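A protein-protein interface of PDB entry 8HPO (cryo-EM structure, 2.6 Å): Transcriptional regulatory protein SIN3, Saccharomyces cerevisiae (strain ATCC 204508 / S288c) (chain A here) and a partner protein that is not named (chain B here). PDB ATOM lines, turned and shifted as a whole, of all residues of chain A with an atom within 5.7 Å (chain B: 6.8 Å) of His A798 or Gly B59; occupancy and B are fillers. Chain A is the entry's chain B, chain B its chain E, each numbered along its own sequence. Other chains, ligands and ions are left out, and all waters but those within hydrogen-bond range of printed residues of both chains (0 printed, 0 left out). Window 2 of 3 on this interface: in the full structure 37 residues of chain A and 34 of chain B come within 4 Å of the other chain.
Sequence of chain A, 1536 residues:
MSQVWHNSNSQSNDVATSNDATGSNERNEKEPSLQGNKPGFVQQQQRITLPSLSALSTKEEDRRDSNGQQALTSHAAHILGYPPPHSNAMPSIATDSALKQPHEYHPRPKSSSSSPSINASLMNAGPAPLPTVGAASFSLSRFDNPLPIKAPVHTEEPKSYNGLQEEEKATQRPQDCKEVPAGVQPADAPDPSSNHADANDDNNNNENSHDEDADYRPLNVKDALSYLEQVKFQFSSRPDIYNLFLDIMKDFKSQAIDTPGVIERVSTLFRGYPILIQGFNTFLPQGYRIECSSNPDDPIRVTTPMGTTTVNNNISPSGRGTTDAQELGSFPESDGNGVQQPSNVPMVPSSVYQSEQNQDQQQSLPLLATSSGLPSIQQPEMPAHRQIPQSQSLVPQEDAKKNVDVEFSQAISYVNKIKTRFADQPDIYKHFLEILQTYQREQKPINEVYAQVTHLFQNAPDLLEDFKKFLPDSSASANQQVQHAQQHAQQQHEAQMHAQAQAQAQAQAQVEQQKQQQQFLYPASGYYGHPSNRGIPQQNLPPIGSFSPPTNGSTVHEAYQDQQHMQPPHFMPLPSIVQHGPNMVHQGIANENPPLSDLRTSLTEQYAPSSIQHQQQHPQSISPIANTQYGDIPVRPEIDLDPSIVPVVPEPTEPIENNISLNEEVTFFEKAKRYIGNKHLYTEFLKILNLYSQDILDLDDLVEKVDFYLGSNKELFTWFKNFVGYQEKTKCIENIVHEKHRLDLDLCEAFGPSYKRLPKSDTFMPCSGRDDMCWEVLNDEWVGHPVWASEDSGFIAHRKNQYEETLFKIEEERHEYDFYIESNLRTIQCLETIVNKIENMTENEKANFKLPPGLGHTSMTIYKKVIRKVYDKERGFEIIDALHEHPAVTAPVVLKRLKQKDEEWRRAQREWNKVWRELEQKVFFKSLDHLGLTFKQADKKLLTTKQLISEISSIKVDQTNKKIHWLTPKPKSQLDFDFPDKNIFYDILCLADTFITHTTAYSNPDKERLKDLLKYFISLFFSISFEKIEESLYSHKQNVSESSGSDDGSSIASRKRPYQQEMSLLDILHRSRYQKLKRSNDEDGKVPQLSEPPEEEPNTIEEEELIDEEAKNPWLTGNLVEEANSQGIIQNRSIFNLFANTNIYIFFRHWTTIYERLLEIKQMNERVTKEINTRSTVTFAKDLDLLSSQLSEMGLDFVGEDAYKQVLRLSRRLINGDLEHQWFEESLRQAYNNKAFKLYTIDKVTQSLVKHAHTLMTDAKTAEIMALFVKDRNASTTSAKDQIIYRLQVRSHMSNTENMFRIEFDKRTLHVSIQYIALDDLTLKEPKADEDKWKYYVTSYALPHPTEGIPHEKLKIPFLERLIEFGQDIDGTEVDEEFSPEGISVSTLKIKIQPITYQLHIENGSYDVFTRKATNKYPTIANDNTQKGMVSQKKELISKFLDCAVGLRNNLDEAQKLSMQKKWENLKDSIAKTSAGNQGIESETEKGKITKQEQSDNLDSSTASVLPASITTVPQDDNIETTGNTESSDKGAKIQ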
ATOM      1  N   ILE A 796     -11.831 -24.621   9.164  1.00  0.00           N
ATOM      2  CA  ILE A 796     -12.614 -24.327  10.357  1.00  0.00           C
ATOM      3  C   ILE A 796     -12.212 -25.314  11.443  1.00  0.00           C
ATOM      4  O   ILE A 796     -11.706 -26.405  11.160  1.00  0.00           O
ATOM      5  CB  ILE A 796     -14.127 -24.390  10.055  1.00  0.00           C
ATOM      6  CG1 ILE A 796     -14.950 -23.958  11.269  1.00  0.00           C
ATOM      7  CG2 ILE A 796     -14.519 -25.795   9.648  1.00  0.00           C
ATOM      8  CD1 ILE A 796     -14.567 -22.594  11.814  1.00  0.00           C
ATOM      9  N   ALA A 797     -12.433 -24.935  12.699  1.00  0.00           N
ATOM     10  CA  ALA A 797     -12.105 -25.803  13.820  1.00  0.00           C
ATOM     11  C   ALA A 797     -13.338 -26.580  14.256  1.00  0.00           C
ATOM     12  O   ALA A 797     -14.442 -26.030  14.313  1.00  0.00           O
ATOM     13  CB  ALA A 797     -11.555 -24.985  14.987  1.00  0.00           C
ATOM     14  N   HIS A 798     -13.145 -27.861  14.554  1.00  0.00           N
ATOM     15  CA  HIS A 798     -14.219 -28.681  15.092  1.00  0.00           C
ATOM     16  C   HIS A 798     -14.720 -28.090  16.404  1.00  0.00           C
ATOM     17  O   HIS A 798     -13.948 -27.520  17.180  1.00  0.00           O
ATOM     18  CB  HIS A 798     -13.728 -30.115  15.300  1.00  0.00           C
ATOM     19  CG  HIS A 798     -14.788 -31.058  15.779  1.00  0.00           C
ATOM     20  ND1 HIS A 798     -14.756 -31.639  17.029  1.00  0.00           N
ATOM     21  CD2 HIS A 798     -15.908 -31.522  15.177  1.00  0.00           C
ATOM     22  CE1 HIS A 798     -15.812 -32.419  17.176  1.00  0.00           C
ATOM     23  NE2 HIS A 798     -16.526 -32.366  16.066  1.00  0.00           N
ATOM     24  N   ARG A 799     -16.020 -28.214  16.645  1.00  0.00           N
ATOM     25  CA  ARG A 799     -16.629 -27.694  17.856  1.00  0.00           C
ATOM     26  C   ARG A 799     -17.694 -28.659  18.349  1.00  0.00           C
ATOM     27  O   ARG A 799     -18.415 -29.280  17.564  1.00  0.00           O
ATOM     28  CB  ARG A 799     -17.224 -26.301  17.632  1.00  0.00           C
ATOM     29  CG  ARG A 799     -16.181 -25.194  17.562  1.00  0.00           C
ATOM     30  CD  ARG A 799     -16.625 -23.964  18.332  1.00  0.00           C
ATOM     31  NE  ARG A 799     -18.068 -23.950  18.525  1.00  0.00           N
ATOM     32  CZ  ARG A 799     -18.919 -23.335  17.715  1.00  0.00           C
ATOM     33  NH1 ARG A 799     -20.218 -23.380  17.958  1.00  0.00           N
ATOM     34  NH2 ARG A 799     -18.468 -22.672  16.660  1.00  0.00           N
ATOM     35  N   LYS A 800     -17.792 -28.762  19.670  1.00  0.00           N
ATOM     36  CA  LYS A 800     -18.561 -29.817  20.311  1.00  0.00           C
ATOM     37  C   LYS A 800     -20.059 -29.635  20.112  1.00  0.00           C
ATOM     38  O   LYS A 800     -20.614 -28.550  20.301  1.00  0.00           O
ATOM     39  CB  LYS A 800     -18.255 -29.878  21.808  1.00  0.00           C
ATOM     40  CG  LYS A 800     -16.843 -30.314  22.150  1.00  0.00           C
ATOM     41  CD  LYS A 800     -16.315 -31.343  21.170  1.00  0.00           C
ATOM     42  CE  LYS A 800     -14.859 -31.691  21.451  1.00  0.00           C
ATOM     43  NZ  LYS A 800     -14.717 -32.767  22.466  1.00  0.00           N
ATOM     44  N   GLU A 804     -22.860 -33.738  23.672  1.00  0.00           N
ATOM     45  CA  GLU A 804     -21.567 -34.184  24.168  1.00  0.00           C
ATOM     46  C   GLU A 804     -21.195 -33.462  25.454  1.00  0.00           C
ATOM     47  O   GLU A 804     -20.644 -34.067  26.382  1.00  0.00           O
ATOM     48  CB  GLU A 804     -20.504 -33.954  23.103  1.00  0.00           C
ATOM     49  CG  GLU A 804     -20.566 -34.942  21.971  1.00  0.00           C
ATOM     50  CD  GLU A 804     -19.364 -34.852  21.064  1.00  0.00           C
ATOM     51  OE1 GLU A 804     -18.936 -33.723  20.767  1.00  0.00           O
ATOM     52  OE2 GLU A 804     -18.845 -35.908  20.651  1.00  0.00           O
ATOM     53  N   GLU A 805     -21.488 -32.166  25.528  1.00  0.00           N
ATOM     54  CA  GLU A 805     -21.131 -31.394  26.709  1.00  0.00           C
ATOM     55  C   GLU A 805     -21.961 -31.797  27.915  1.00  0.00           C
ATOM     56  O   GLU A 805     -21.446 -31.843  29.038  1.00  0.00           O
ATOM     57  CB  GLU A 805     -21.287 -29.911  26.420  1.00  0.00           C
ATOM     58  CG  GLU A 805     -20.606 -29.504  25.154  1.00  0.00           C
ATOM     59  CD  GLU A 805     -20.058 -28.111  25.250  1.00  0.00           C
ATOM     60  OE1 GLU A 805     -19.031 -27.953  25.939  1.00  0.00           O
ATOM     61  OE2 GLU A 805     -20.631 -27.185  24.640  1.00  0.00           O
ATOM     62  N   HIS A 930     -23.531 -35.825  14.309  1.00  0.00           N
ATOM     63  CA  HIS A 930     -23.075 -34.443  14.346  1.00  0.00           C
ATOM     64  C   HIS A 930     -23.594 -33.664  13.147  1.00  0.00           C
ATOM     65  O   HIS A 930     -23.966 -32.493  13.268  1.00  0.00           O
ATOM     66  CB  HIS A 930     -21.548 -34.408  14.400  1.00  0.00           C
ATOM     67  CG  HIS A 930     -20.985 -33.067  14.743  1.00  0.00           C
ATOM     68  ND1 HIS A 930     -21.169 -32.475  15.972  1.00  0.00           N
ATOM     69  CD2 HIS A 930     -20.242 -32.201  14.015  1.00  0.00           C
ATOM     70  CE1 HIS A 930     -20.565 -31.301  15.988  1.00  0.00           C
ATOM     71  NE2 HIS A 930     -19.995 -31.110  14.812  1.00  0.00           N
ATOM     72  N   GLU B  56     -21.398 -20.565  22.044  1.00  0.00           N
ATOM     73  CA  GLU B  56     -20.491 -20.862  23.146  1.00  0.00           C
ATOM     74  C   GLU B  56     -19.177 -21.432  22.634  1.00  0.00           C
ATOM     75  O   GLU B  56     -19.147 -22.137  21.623  1.00  0.00           O
ATOM     76  CB  GLU B  56     -21.151 -21.831  24.121  1.00  0.00           C
ATOM     77  CG  GLU B  56     -22.182 -21.169  25.033  1.00  0.00           C
ATOM     78  CD  GLU B  56     -23.419 -20.700  24.286  1.00  0.00           C
ATOM     79  OE1 GLU B  56     -24.090 -19.761  24.763  1.00  0.00           O
ATOM     80  OE2 GLU B  56     -23.717 -21.273  23.217  1.00  0.00           O
ATOM     81  N   ALA B  57     -18.091 -21.120  23.334  1.00  0.00           N
ATOM     82  CA  ALA B  57     -16.753 -21.413  22.836  1.00  0.00           C
ATOM     83  C   ALA B  57     -16.233 -22.715  23.424  1.00  0.00           C
ATOM     84  O   ALA B  57     -15.210 -22.718  24.114  1.00  0.00           O
ATOM     85  CB  ALA B  57     -15.801 -20.275  23.174  1.00  0.00           C
ATOM     86  N   THR B  58     -16.906 -23.820  23.123  1.00  0.00           N
ATOM     87  CA  THR B  58     -16.484 -25.116  23.626  1.00  0.00           C
ATOM     88  C   THR B  58     -16.030 -25.973  22.458  1.00  0.00           C
ATOM     89  O   THR B  58     -16.802 -26.226  21.530  1.00  0.00           O
ATOM     90  CB  THR B  58     -17.608 -25.817  24.380  1.00  0.00           C
ATOM     91  OG1 THR B  58     -18.586 -26.273  23.440  1.00  0.00           O
ATOM     92  CG2 THR B  58     -18.260 -24.875  25.371  1.00  0.00           C
ATOM     93  N   GLY B  59     -14.784 -26.420  22.522  1.00  0.00           N
ATOM     94  CA  GLY B  59     -14.178 -27.151  21.438  1.00  0.00           C
ATOM     95  C   GLY B  59     -13.019 -26.449  20.777  1.00  0.00           C
ATOM     96  O   GLY B  59     -12.237 -27.103  20.080  1.00  0.00           O
ATOM     97  N   ILE B  60     -12.874 -25.154  20.981  1.00  0.00           N
ATOM     98  CA  ILE B  60     -11.777 -24.392  20.400  1.00  0.00           C
ATOM     99  C   ILE B  60     -10.499 -24.690  21.168  1.00  0.00           C
ATOM    100  O   ILE B  60     -10.524 -24.906  22.382  1.00  0.00           O
ATOM    101  CB  ILE B  60     -12.097 -22.886  20.409  1.00  0.00           C
ATOM    102  CG1 ILE B  60     -12.747 -22.487  21.729  1.00  0.00           C
ATOM    103  CG2 ILE B  60     -13.004 -22.533  19.259  1.00  0.00           C
ATOM    104  CD1 ILE B  60     -12.379 -21.103  22.180  1.00  0.00           C
ATOM    105  N   SER B  61      -9.375 -24.706  20.456  1.00  0.00           N
ATOM    106  CA  SER B  61      -8.076 -24.930  21.079  1.00  0.00           C
ATOM    107  C   SER B  61      -7.306 -23.623  21.230  1.00  0.00           C
ATOM    108  O   SER B  61      -6.805 -23.310  22.312  1.00  0.00           O
ATOM    109  CB  SER B  61      -7.263 -25.939  20.264  1.00  0.00           C
ATOM    110  OG  SER B  61      -6.303 -25.282  19.460  1.00  0.00           O
ATOM    111  N   SER B  62      -7.198 -22.857  20.150  1.00  0.00           N
ATOM    112  CA  SER B  62      -6.562 -21.552  20.199  1.00  0.00           C
ATOM    113  C   SER B  62      -7.582 -20.485  20.576  1.00  0.00           C
ATOM    114  O   SER B  62      -8.741 -20.767  20.884  1.00  0.00           O
ATOM    115  CB  SER B  62      -5.909 -21.225  18.861  1.00  0.00           C
ATOM    116  OG  SER B  62      -5.314 -19.943  18.884  1.00  0.00           O
ATOM    117  N   ASN B  82      -8.293 -27.319  27.507  1.00  0.00           N
ATOM    118  CA  ASN B  82      -9.354 -26.536  26.876  1.00  0.00           C
ATOM    119  C   ASN B  82     -10.701 -27.094  27.309  1.00  0.00           C
ATOM    120  O   ASN B  82     -11.467 -27.595  26.486  1.00  0.00           O
ATOM    121  CB  ASN B  82      -9.221 -26.561  25.361  1.00  0.00           C
ATOM    122  CG  ASN B  82      -7.792 -26.571  24.905  1.00  0.00           C
ATOM    123  OD1 ASN B  82      -6.920 -25.990  25.547  1.00  0.00           O
ATOM    124  ND2 ASN B  82      -7.535 -27.235  23.787  1.00  0.00           N
ATOM    125  N   PRO B  85     -14.388 -23.813  29.744  1.00  0.00           N
ATOM    126  CA  PRO B  85     -15.746 -23.363  29.415  1.00  0.00           C
ATOM    127  C   PRO B  85     -16.880 -24.250  29.914  1.00  0.00           C
ATOM    128  O   PRO B  85     -18.047 -23.903  29.723  1.00  0.00           O
ATOM    129  CB  PRO B  85     -15.720 -23.321  27.886  1.00  0.00           C
ATOM    130  CG  PRO B  85     -14.343 -22.938  27.570  1.00  0.00           C
ATOM    131  CD  PRO B  85     -13.472 -23.576  28.610  1.00  0.00           C
ATOM    132  N   MET B  86     -16.585 -25.377  30.561  1.00  0.00           N
ATOM    133  CA  MET B  86     -17.654 -26.273  30.991  1.00  0.00           C
ATOM    134  C   MET B  86     -17.750 -26.420  32.503  1.00  0.00           C
ATOM    135  O   MET B  86     -17.896 -27.537  33.001  1.00  0.00           O
ATOM    136  CB  MET B  86     -17.483 -27.661  30.379  1.00  0.00           C
ATOM    137  CG  MET B  86     -16.926 -27.690  28.977  1.00  0.00           C
ATOM    138  SD  MET B  86     -16.986 -29.365  28.318  1.00  0.00           S
ATOM    139  CE  MET B  86     -15.812 -29.256  26.978  1.00  0.00           C
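Among the printed residues, pairs that only touch across the chains: Arg A799 with Glu B56 (3.7 Å) and Arg A799 with Thr B58 (3.9 Å).
Of the 8 printed residues of chain A, 4 touch a printed residue of chain B.
Among the printed residues, 6 pairs touch across the chains.
Among the printed residues, no Asp or Glu carboxylate lies within 4 Å of a Lys or Arg side-chain nitrogen of the other chain.
Of chain B, only Gly B59 comes within 4 Å of His A798.
Of chain A, only His A798 (3.4 Å) comes within 4 Å of Gly B59.
Of the printed residues of chain A, Glu B56 touches Arg A799 (3.7 Å).
Of the printed residues of chain B, Arg A799 touches Glu B56 and Thr B58.
Printed residues of chain B within 4 Å of Glu A805: Thr B58 and Met B86.
Ile A796 touches none of the printed residues of chain B.
His A930 touches none of the printed residues of chain B.
The backbone carbonyl oxygen (O) of Thr B58 lies within hydrogen-bond range of the backbone NH (N) of Lys A800 (3.3 Å).
OG1 of Thr B58 is in hydrogen-bond range of OE2 of Glu A805.
The backbone carbonyl oxygen (O) of His A798 sits close to the backbone carbonyl oxygen (O) of Gly B59, at 3.4 Å.
The side-chain sulfur of Met B86 lies close to the side-chain carboxylate of Glu A805 (3.4 Å).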
